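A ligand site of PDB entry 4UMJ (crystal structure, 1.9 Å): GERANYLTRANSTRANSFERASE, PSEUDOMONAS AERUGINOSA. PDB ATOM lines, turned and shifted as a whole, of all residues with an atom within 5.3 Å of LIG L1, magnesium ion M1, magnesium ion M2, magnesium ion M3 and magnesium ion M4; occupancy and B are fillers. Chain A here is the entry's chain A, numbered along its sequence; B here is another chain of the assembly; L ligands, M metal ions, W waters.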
ATOM      1  N   ARG A  48     -25.172  19.562  25.375  1.00  0.00           N
ATOM      2  CA  ARG A  48     -24.415  20.321  26.347  1.00  0.00           C
ATOM      3  C   ARG A  48     -25.285  21.330  27.084  1.00  0.00           C
ATOM      4  O   ARG A  48     -25.213  21.428  28.322  1.00  0.00           O
ATOM      5  CB  ARG A  48     -23.207  20.918  25.675  1.00  0.00           C
ATOM      6  CG  ARG A  48     -22.147  19.862  25.450  1.00  0.00           C
ATOM      7  CD  ARG A  48     -21.164  20.208  24.329  1.00  0.00           C
ATOM      8  NE  ARG A  48     -20.400  19.048  23.918  1.00  0.00           N
ATOM      9  CZ  ARG A  48     -20.824  18.147  23.030  1.00  0.00           C
ATOM     10  NH1 ARG A  48     -22.002  18.277  22.419  1.00  0.00           N
ATOM     11  NH2 ARG A  48     -20.032  17.156  22.740  1.00  0.00           N
ATOM     12  N   HIS A  77     -19.071  24.335  21.412  1.00  0.00           N
ATOM     13  CA  HIS A  77     -19.275  23.082  20.675  1.00  0.00           C
ATOM     14  C   HIS A  77     -19.379  23.367  19.149  1.00  0.00           C
ATOM     15  O   HIS A  77     -18.734  22.719  18.296  1.00  0.00           O
ATOM     16  CB  HIS A  77     -20.487  22.354  21.250  1.00  0.00           C
ATOM     17  CG  HIS A  77     -20.800  21.084  20.541  1.00  0.00           C
ATOM     18  ND1 HIS A  77     -19.891  20.070  20.397  1.00  0.00           N
ATOM     19  CD2 HIS A  77     -21.881  20.737  19.813  1.00  0.00           C
ATOM     20  CE1 HIS A  77     -20.435  19.091  19.693  1.00  0.00           C
ATOM     21  NE2 HIS A  77     -21.641  19.498  19.294  1.00  0.00           N
ATOM     22  N   SER A  80     -16.203  24.421  17.446  1.00  0.00           N
ATOM     23  CA  SER A  80     -15.323  23.242  17.333  1.00  0.00           C
ATOM     24  C   SER A  80     -15.666  22.320  16.138  1.00  0.00           C
ATOM     25  O   SER A  80     -14.751  21.785  15.533  1.00  0.00           O
ATOM     26  CB  SER A  80     -15.339  22.394  18.600  1.00  0.00           C
ATOM     27  OG  SER A  80     -16.450  21.532  18.730  1.00  0.00           O
ATOM     28  N   LEU A  81     -16.969  22.156  15.859  1.00  0.00           N
ATOM     29  CA  LEU A  81     -17.415  21.379  14.704  1.00  0.00           C
ATOM     30  C   LEU A  81     -16.921  22.030  13.410  1.00  0.00           C
ATOM     31  O   LEU A  81     -16.480  21.345  12.550  1.00  0.00           O
ATOM     32  CB  LEU A  81     -18.934  21.253  14.642  1.00  0.00           C
ATOM     33  CG  LEU A  81     -19.527  20.537  15.873  1.00  0.00           C
ATOM     34  CD1 LEU A  81     -21.029  20.272  15.710  1.00  0.00           C
ATOM     35  CD2 LEU A  81     -18.842  19.244  16.240  1.00  0.00           C
ATOM     36  N   ASP A  84     -13.298  21.343  13.077  1.00  0.00           N
ATOM     37  CA  ASP A  84     -13.102  19.881  12.916  1.00  0.00           C
ATOM     38  C   ASP A  84     -13.423  19.428  11.473  1.00  0.00           C
ATOM     39  O   ASP A  84     -12.760  18.538  10.992  1.00  0.00           O
ATOM     40  CB  ASP A  84     -13.964  19.155  13.922  1.00  0.00           C
ATOM     41  CG  ASP A  84     -13.883  17.672  13.822  1.00  0.00           C
ATOM     42  OD1 ASP A  84     -12.881  17.058  14.262  1.00  0.00           O
ATOM     43  OD2 ASP A  84     -14.856  17.095  13.311  1.00  0.00           O
ATOM     44  N   ASP A  85     -14.371  20.079  10.805  1.00  0.00           N
ATOM     45  CA  ASP A  85     -14.842  19.694   9.464  1.00  0.00           C
ATOM     46  C   ASP A  85     -13.908  20.175   8.379  1.00  0.00           C
ATOM     47  O   ASP A  85     -13.934  19.663   7.236  1.00  0.00           O
ATOM     48  CB  ASP A  85     -16.221  20.240   9.187  1.00  0.00           C
ATOM     49  CG  ASP A  85     -17.298  19.489   9.899  1.00  0.00           C
ATOM     50  OD1 ASP A  85     -17.092  18.286  10.159  1.00  0.00           O
ATOM     51  OD2 ASP A  85     -18.382  20.091  10.120  1.00  0.00           O
ATOM     52  N   ASP A  90     -10.864  16.990   9.513  1.00  0.00           N
ATOM     53  CA  ASP A  90     -11.652  15.811   9.062  1.00  0.00           C
ATOM     54  C   ASP A  90     -12.141  15.912   7.592  1.00  0.00           C
ATOM     55  O   ASP A  90     -12.588  14.931   7.039  1.00  0.00           O
ATOM     56  CB  ASP A  90     -12.811  15.482   9.986  1.00  0.00           C
ATOM     57  CG  ASP A  90     -12.379  15.010  11.298  1.00  0.00           C
ATOM     58  OD1 ASP A  90     -11.211  14.614  11.422  1.00  0.00           O
ATOM     59  OD2 ASP A  90     -13.186  15.018  12.276  1.00  0.00           O
ATOM     60  N   ASP A  92     -14.796  17.167   5.926  1.00  0.00           N
ATOM     61  CA  ASP A  92     -16.109  16.692   5.695  1.00  0.00           C
ATOM     62  C   ASP A  92     -16.902  17.706   4.889  1.00  0.00           C
ATOM     63  O   ASP A  92     -16.916  18.885   5.191  1.00  0.00           O
ATOM     64  CB  ASP A  92     -16.811  16.380   6.998  1.00  0.00           C
ATOM     65  CG  ASP A  92     -16.448  14.974   7.526  1.00  0.00           C
ATOM     66  OD1 ASP A  92     -16.431  14.047   6.693  1.00  0.00           O
ATOM     67  OD2 ASP A  92     -16.127  14.801   8.704  1.00  0.00           O
ATOM     68  N   ARG A  95     -22.469  17.607   7.262  1.00  0.00           N
ATOM     69  CA  ARG A  95     -22.721  17.391   8.681  1.00  0.00           C
ATOM     70  C   ARG A  95     -24.232  17.325   8.790  1.00  0.00           C
ATOM     71  O   ARG A  95     -24.932  18.261   8.372  1.00  0.00           O
ATOM     72  CB  ARG A  95     -22.151  18.553   9.524  1.00  0.00           C
ATOM     73  CG  ARG A  95     -22.466  18.477  10.995  1.00  0.00           C
ATOM     74  CD  ARG A  95     -21.600  19.407  11.849  1.00  0.00           C
ATOM     75  NE  ARG A  95     -20.215  18.960  11.937  1.00  0.00           N
ATOM     76  CZ  ARG A  95     -19.788  17.927  12.661  1.00  0.00           C
ATOM     77  NH1 ARG A  95     -20.637  17.193  13.356  1.00  0.00           N
ATOM     78  NH2 ARG A  95     -18.490  17.620  12.685  1.00  0.00           N
ATOM     79  N   MET A 154     -10.432  20.750  25.348  1.00  0.00           N
ATOM     80  CA  MET A 154     -10.997  20.376  24.087  1.00  0.00           C
ATOM     81  C   MET A 154     -10.019  20.479  22.911  1.00  0.00           C
ATOM     82  O   MET A 154      -9.882  19.520  22.117  1.00  0.00           O
ATOM     83  CB  MET A 154     -12.230  21.218  23.764  1.00  0.00           C
ATOM     84  CG  MET A 154     -12.940  20.855  22.481  1.00  0.00           C
ATOM     85  SD  MET A 154     -14.241  22.023  22.023  1.00  0.00           S
ATOM     86  CE  MET A 154     -13.319  23.500  21.468  1.00  0.00           C
ATOM     87  N   VAL A 155      -9.383  21.627  22.771  1.00  0.00           N
ATOM     88  CA  VAL A 155      -8.415  21.792  21.688  1.00  0.00           C
ATOM     89  C   VAL A 155      -7.217  20.863  21.850  1.00  0.00           C
ATOM     90  O   VAL A 155      -6.747  20.282  20.871  1.00  0.00           O
ATOM     91  CB  VAL A 155      -7.979  23.246  21.525  1.00  0.00           C
ATOM     92  CG1 VAL A 155      -6.753  23.387  20.645  1.00  0.00           C
ATOM     93  CG2 VAL A 155      -9.134  24.057  20.935  1.00  0.00           C
ATOM     94  N   GLN A 158      -8.324  17.408  20.503  1.00  0.00           N
ATOM     95  CA  GLN A 158      -8.174  17.419  19.059  1.00  0.00           C
ATOM     96  C   GLN A 158      -6.742  17.150  18.615  1.00  0.00           C
ATOM     97  O   GLN A 158      -6.479  16.298  17.693  1.00  0.00           O
ATOM     98  CB  GLN A 158      -8.701  18.718  18.495  1.00  0.00           C
ATOM     99  CG  GLN A 158      -8.849  18.665  17.015  1.00  0.00           C
ATOM    100  CD  GLN A 158     -10.069  17.905  16.546  1.00  0.00           C
ATOM    101  OE1 GLN A 158     -10.659  17.053  17.270  1.00  0.00           O
ATOM    102  NE2 GLN A 158     -10.455  18.184  15.351  1.00  0.00           N
ATOM    103  N   ASP A 161      -5.690  13.523  19.392  1.00  0.00           N
ATOM    104  CA  ASP A 161      -6.264  12.701  18.383  1.00  0.00           C
ATOM    105  C   ASP A 161      -5.405  12.744  17.106  1.00  0.00           C
ATOM    106  O   ASP A 161      -4.940  11.702  16.630  1.00  0.00           O
ATOM    107  CB  ASP A 161      -7.715  13.143  18.119  1.00  0.00           C
ATOM    108  CG  ASP A 161      -8.322  12.474  16.910  1.00  0.00           C
ATOM    109  OD1 ASP A 161      -7.626  12.508  15.865  1.00  0.00           O
ATOM    110  OD2 ASP A 161      -9.463  11.953  17.000  1.00  0.00           O
ATOM    111  N   LYS A 181     -10.939  15.551  24.490  1.00  0.00           N
ATOM    112  CA  LYS A 181     -11.603  15.943  23.252  1.00  0.00           C
ATOM    113  C   LYS A 181     -13.093  16.208  23.446  1.00  0.00           C
ATOM    114  O   LYS A 181     -13.641  17.163  22.906  1.00  0.00           O
ATOM    115  CB  LYS A 181     -11.340  14.914  22.129  1.00  0.00           C
ATOM    116  CG  LYS A 181     -11.616  15.482  20.770  1.00  0.00           C
ATOM    117  CD  LYS A 181     -11.219  14.523  19.647  1.00  0.00           C
ATOM    118  CE  LYS A 181     -12.150  13.364  19.534  1.00  0.00           C
ATOM    119  NZ  LYS A 181     -11.710  12.541  18.384  1.00  0.00           N
ATOM    120  N   THR A 182     -13.751  15.423  24.301  1.00  0.00           N
ATOM    121  CA  THR A 182     -15.131  15.667  24.628  1.00  0.00           C
ATOM    122  C   THR A 182     -15.439  15.808  26.133  1.00  0.00           C
ATOM    123  O   THR A 182     -16.362  16.536  26.475  1.00  0.00           O
ATOM    124  CB  THR A 182     -16.075  14.615  24.019  1.00  0.00           C
ATOM    125  OG1 THR A 182     -15.592  13.308  24.229  1.00  0.00           O
ATOM    126  CG2 THR A 182     -16.243  14.821  22.522  1.00  0.00           C
ATOM    127  N   LEU B 112      -5.410  24.928  15.504  1.00  0.00           N
ATOM    128  CA  LEU B 112      -5.658  24.573  16.885  1.00  0.00           C
ATOM    129  C   LEU B 112      -4.855  25.391  17.883  1.00  0.00           C
ATOM    130  O   LEU B 112      -5.386  25.854  18.852  1.00  0.00           O
ATOM    131  CB  LEU B 112      -5.307  23.091  17.145  1.00  0.00           C
ATOM    132  CG  LEU B 112      -6.172  22.106  16.338  1.00  0.00           C
ATOM    133  CD1 LEU B 112      -5.697  20.679  16.488  1.00  0.00           C
ATOM    134  CD2 LEU B 112      -7.640  22.269  16.666  1.00  0.00           C
HETATM  135  P1  LIG L   1     -15.270  13.835  15.893  1.00  0.00           P
HETATM  136  O1  LIG L   1     -14.556  14.379  14.681  1.00  0.00           O
HETATM  137  O2  LIG L   1     -15.687  12.400  15.691  1.00  0.00           O
HETATM  138  O3  LIG L   1     -14.407  14.152  17.124  1.00  0.00           O
HETATM  139  C1  LIG L   1     -16.862  14.729  16.060  1.00  0.00           C
HETATM  140  P2  LIG L   1     -17.771  14.403  14.491  1.00  0.00           P
HETATM  141  O4  LIG L   1     -17.052  15.011  13.333  1.00  0.00           O
HETATM  142  O5  LIG L   1     -19.060  15.139  14.572  1.00  0.00           O
HETATM  143  O6  LIG L   1     -18.115  12.927  14.414  1.00  0.00           O
HETATM  144  O7  LIG L   1     -17.513  14.214  17.173  1.00  0.00           O
HETATM  145  C2  LIG L   1     -16.717  16.217  16.254  1.00  0.00           C
HETATM  146  C3  LIG L   1     -15.633  16.733  17.187  1.00  0.00           C
HETATM  147  N1  LIG L   1     -15.743  16.400  18.622  1.00  0.00           N
HETATM  148  C4  LIG L   1     -14.611  17.125  19.250  1.00  0.00           C
HETATM  149  C5  LIG L   1     -14.382  18.538  18.674  1.00  0.00           C
HETATM  150  C6  LIG L   1     -13.236  19.294  19.284  1.00  0.00           C
HETATM  151  C7  LIG L   1     -12.531  19.982  18.120  1.00  0.00           C
HETATM  152  C8  LIG L   1     -11.736  21.195  18.452  1.00  0.00           C
HETATM  153  C9  LIG L   1     -17.038  16.910  19.071  1.00  0.00           C
HETATM  154  P1  LG2 L   2     -19.664  11.654  17.289  1.00  0.00           P
HETATM  155  O1  LG2 L   2     -20.319  12.831  16.668  1.00  0.00           O
HETATM  156  O2  LG2 L   2     -18.200  11.461  16.975  1.00  0.00           O
HETATM  157  O3  LG2 L   2     -19.879  11.646  18.735  1.00  0.00           O
HETATM  158  C1  LG2 L   2     -20.647  10.261  16.627  1.00  0.00           C
HETATM  159  P2  LG2 L   2     -20.283  10.268  14.852  1.00  0.00           P
HETATM  160  O4  LG2 L   2     -20.954  11.457  14.200  1.00  0.00           O
HETATM  161  O5  LG2 L   2     -21.019   9.167  14.124  1.00  0.00           O
HETATM  162  O6  LG2 L   2     -18.833  10.060  14.487  1.00  0.00           O
HETATM  163  O7  LG2 L   2     -20.206   9.086  17.268  1.00  0.00           O
HETATM  164  C2  LG2 L   2     -22.117  10.620  16.728  1.00  0.00           C
HETATM  165  C3  LG2 L   2     -22.760  10.667  18.101  1.00  0.00           C
HETATM  166  N1  LG2 L   2     -22.590  11.849  18.972  1.00  0.00           N
HETATM  167  C4  LG2 L   2     -23.310  11.478  20.237  1.00  0.00           C
HETATM  168  C5  LG2 L   2     -23.065  12.467  21.393  1.00  0.00           C
HETATM  169  C6  LG2 L   2     -21.734  12.188  22.043  1.00  0.00           C
HETATM  170  C7  LG2 L   2     -21.478  13.230  23.107  1.00  0.00           C
HETATM  171  C8  LG2 L   2     -20.000  13.112  23.514  1.00  0.00           C
HETATM  172  C9  LG2 L   2     -23.163  13.035  18.359  1.00  0.00           C
HETATM  173  P1  LG3 L   3     -15.088   8.865  15.496  1.00  0.00           P
HETATM  174  O1  LG3 L   3     -16.372   9.616  15.831  1.00  0.00           O
HETATM  175  O2  LG3 L   3     -14.094   8.754  16.609  1.00  0.00           O
HETATM  176  O3  LG3 L   3     -15.399   7.491  14.947  1.00  0.00           O
HETATM  177  C1  LG3 L   3     -14.196   9.702  14.124  1.00  0.00           C
HETATM  178  P2  LG3 L   3     -15.359  10.014  12.782  1.00  0.00           P
HETATM  179  O4  LG3 L   3     -16.013   8.679  12.442  1.00  0.00           O
HETATM  180  O5  LG3 L   3     -14.649  10.461  11.541  1.00  0.00           O
HETATM  181  O6  LG3 L   3     -16.470  10.969  13.106  1.00  0.00           O
HETATM  182  O7  LG3 L   3     -13.633  10.887  14.640  1.00  0.00           O
HETATM  183  C2  LG3 L   3     -13.125   8.787  13.586  1.00  0.00           C
HETATM  184  C3  LG3 L   3     -11.886   8.941  14.430  1.00  0.00           C
HETATM  185  N1  LG3 L   3     -11.737   7.872  15.424  1.00  0.00           N
HETATM  186  C4  LG3 L   3     -10.784   8.182  16.545  1.00  0.00           C
HETATM  187  C5  LG3 L   3      -9.421   8.847  16.204  1.00  0.00           C
HETATM  188  C6  LG3 L   3      -8.495   8.174  15.175  1.00  0.00           C
HETATM  189  C7  LG3 L   3      -8.776   8.661  13.719  1.00  0.00           C
HETATM  190  C8  LG3 L   3      -7.583   8.793  12.750  1.00  0.00           C
HETATM  191  C9  LG3 L   3     -11.466   6.588  14.787  1.00  0.00           C
HETATM  192 MG    MG M   1     -12.649  14.948  14.333  1.00  0.00          MG
HETATM  193 MG    MG M   2     -15.274  15.192  12.708  1.00  0.00          MG
HETATM  194 MG    MG M   3     -17.131  11.319  15.089  1.00  0.00          MG
HETATM  195 MG    MG M   4     -20.537  13.406  14.778  1.00  0.00          MG
HETATM  196 MG    MG M   5     -16.351   6.801  13.405  1.00  0.00          MG
HETATM  197 MG    MG M   6     -17.135   8.663  19.560  1.00  0.00          MG
HETATM  198  O   HOH W   1     -15.869  15.975  10.869  1.00  0.00           O
HETATM  199  O   HOH W   2     -15.285  13.120  11.934  1.00  0.00           O
HETATM  200  O   HOH W   3     -22.305  14.210  14.884  1.00  0.00           O
HETATM  201  O   HOH W   4     -15.493  13.440  19.647  1.00  0.00           O
HETATM  202  O   HOH W   5     -20.214  15.856  17.602  1.00  0.00           O
HETATM  203  O   HOH W   6     -20.958  13.746  12.797  1.00  0.00           O
HETATM  204  O   HOH W   7     -19.978  15.567  20.240  1.00  0.00           O
HETATM  205  O   HOH W   8     -11.974  12.919  14.281  1.00  0.00           O
HETATM  206  O   HOH W   9     -12.135  15.027  16.342  1.00  0.00           O
HETATM  207  O   HOH W  10     -18.849  11.616  11.814  1.00  0.00           O
HETATM  208  O   HOH W  11     -14.128  11.114  17.694  1.00  0.00           O
HETATM  209  O   HOH W  12     -18.342  13.123  20.079  1.00  0.00           O
HETATM  210  O   HOH W  13     -18.720  14.262  11.168  1.00  0.00           O
HETATM  211  O   HOH W  14     -10.708  15.321  13.941  1.00  0.00           O
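An oxygen (O5) of LIG L1 sits close to the guanidinium group (NH1) of Arg 95 (2.9 Å).
The side-chain amino group of Lys 181 is in salt-bridge range of an oxygen (O3) of LIG L1 (3.4 Å).
No residue comes within 4 Å of magnesium ion M4.
The nearest printed residue that does not touch magnesium ion M4 is Arg 95 (4.05 Å).
Of the 16 residues printed, 2 come within 4 Å of magnesium ion M1.
Magnesium ion M1 is bound by water W14, an oxygen (O1) of LIG L1, water W9, the side-chain carboxylate of Asp 84, the side-chain carboxylate of Asp 90 and water W8.
Magnesium ion M1 has six donor atoms within binding distance.
O4 of LIG L1 is bound to magnesium ion M2 (1.9 Å).
The side-chain carboxylate (OD2) of Asp 84 binds magnesium ion M2 (2.0 Å).
Magnesium ion M2 is bound by water W1 (2.1 Å).
Magnesium ion M2 is bound by the side-chain carboxylate (OD2) of Asp 90, at 2.1 Å.
Water W2 binds magnesium ion M2 (2.2 Å).
An oxygen (O1) of LIG L1 binds magnesium ion M2 (2.3 Å).
Magnesium ion M2 has six donor atoms within binding distance.
Residues that only touch LIG L1: Met 154, Gln 158, Ser 80 and Leu 81.
Hydrophobic or aromatic side chains that line LIG L1: Leu 81 and Met 154.
Of the 16 residues printed, 8 come within 4 Å of LIG L1.
Water W14 bridges OD1 of Asp 90 (2.7 Å) and NE2 of Gln 158 (3.2 Å).
Water W8 lies within hydrogen-bond range of O7 of LG3 L3 (2.6 Å) and OD1 of Asp 90 (3.4 Å).
Water W9 lies within hydrogen-bond range of O3 of LIG L1, OE1 of Gln 158 and NZ of Lys 181.
Water W1 bridges the side-chain carboxylate of Asp 92 and the side-chain carboxylate of Asp 85.
Water W11 lies within hydrogen-bond range of an oxygen (O2) of LG3 L3 (2.6 Å), the side-chain amino group of Lys 181 (2.9 Å) and an oxygen (O3) of LIG L1 (3.1 Å).
Water W12 lies within hydrogen-bond range of O3 of LG2 L2 (2.5 Å) and O7 of LIG L1 (3.2 Å).
Magnesium ion M3 is bound by O2 of LIG L1.
Magnesium ion M3 is bound by O6 of LIG L1, at 2.0 Å.
Magnesium ion M3 is bound by O1 of LG3 L3, 2.0 Å away.
Magnesium ion M3 is bound by O6 of LG3 L3 (2.1 Å).
Magnesium ion M3 is bound by O2 of LG2 L2.
Magnesium ion M3 is bound by O6 of LG2 L2.
Magnesium ion M3 has six donor atoms within binding distance.
Two residues have an atom within 4 Å of magnesium ion M2: Asp 84 and Asp 90.
Magnesium ion M4 is bound by water W3 (1.9 Å), an oxygen (O1) of LG2 L2 (2.0 Å), water W6 (2.1 Å), an oxygen (O4) of LG2 L2 (2.1 Å), an oxygen (O5) of LIG L1 (2.3 Å) and an oxygen (O6) of LIG L1 (2.5 Å).
The side-chain carboxylate (OD2) of Asp 84 sits close to the guanidinium group (NH2) of Arg 95, 3.7 Å away.
NE2 of Gln 158 sits close to OD1 of Asp 84, at 2.9 Å.
The guanidinium group (NE) of Arg 95 lies within salt-bridge range of the side-chain carboxylate (OD2) of Asp 85 (2.8 Å).
NZ of Lys 181 is in salt-bridge range of OD2 of Asp 161 (2.7 Å).
The side-chain hydroxyl of Ser 80 sits at hydrogen-bond distance from the backbone carbonyl oxygen of His 77 (2.6 Å).
No residue comes within 4 Å of magnesium ion M3.
The nearest printed residue that does not touch magnesium ion M3 is Asp 90 (6.1 Å).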
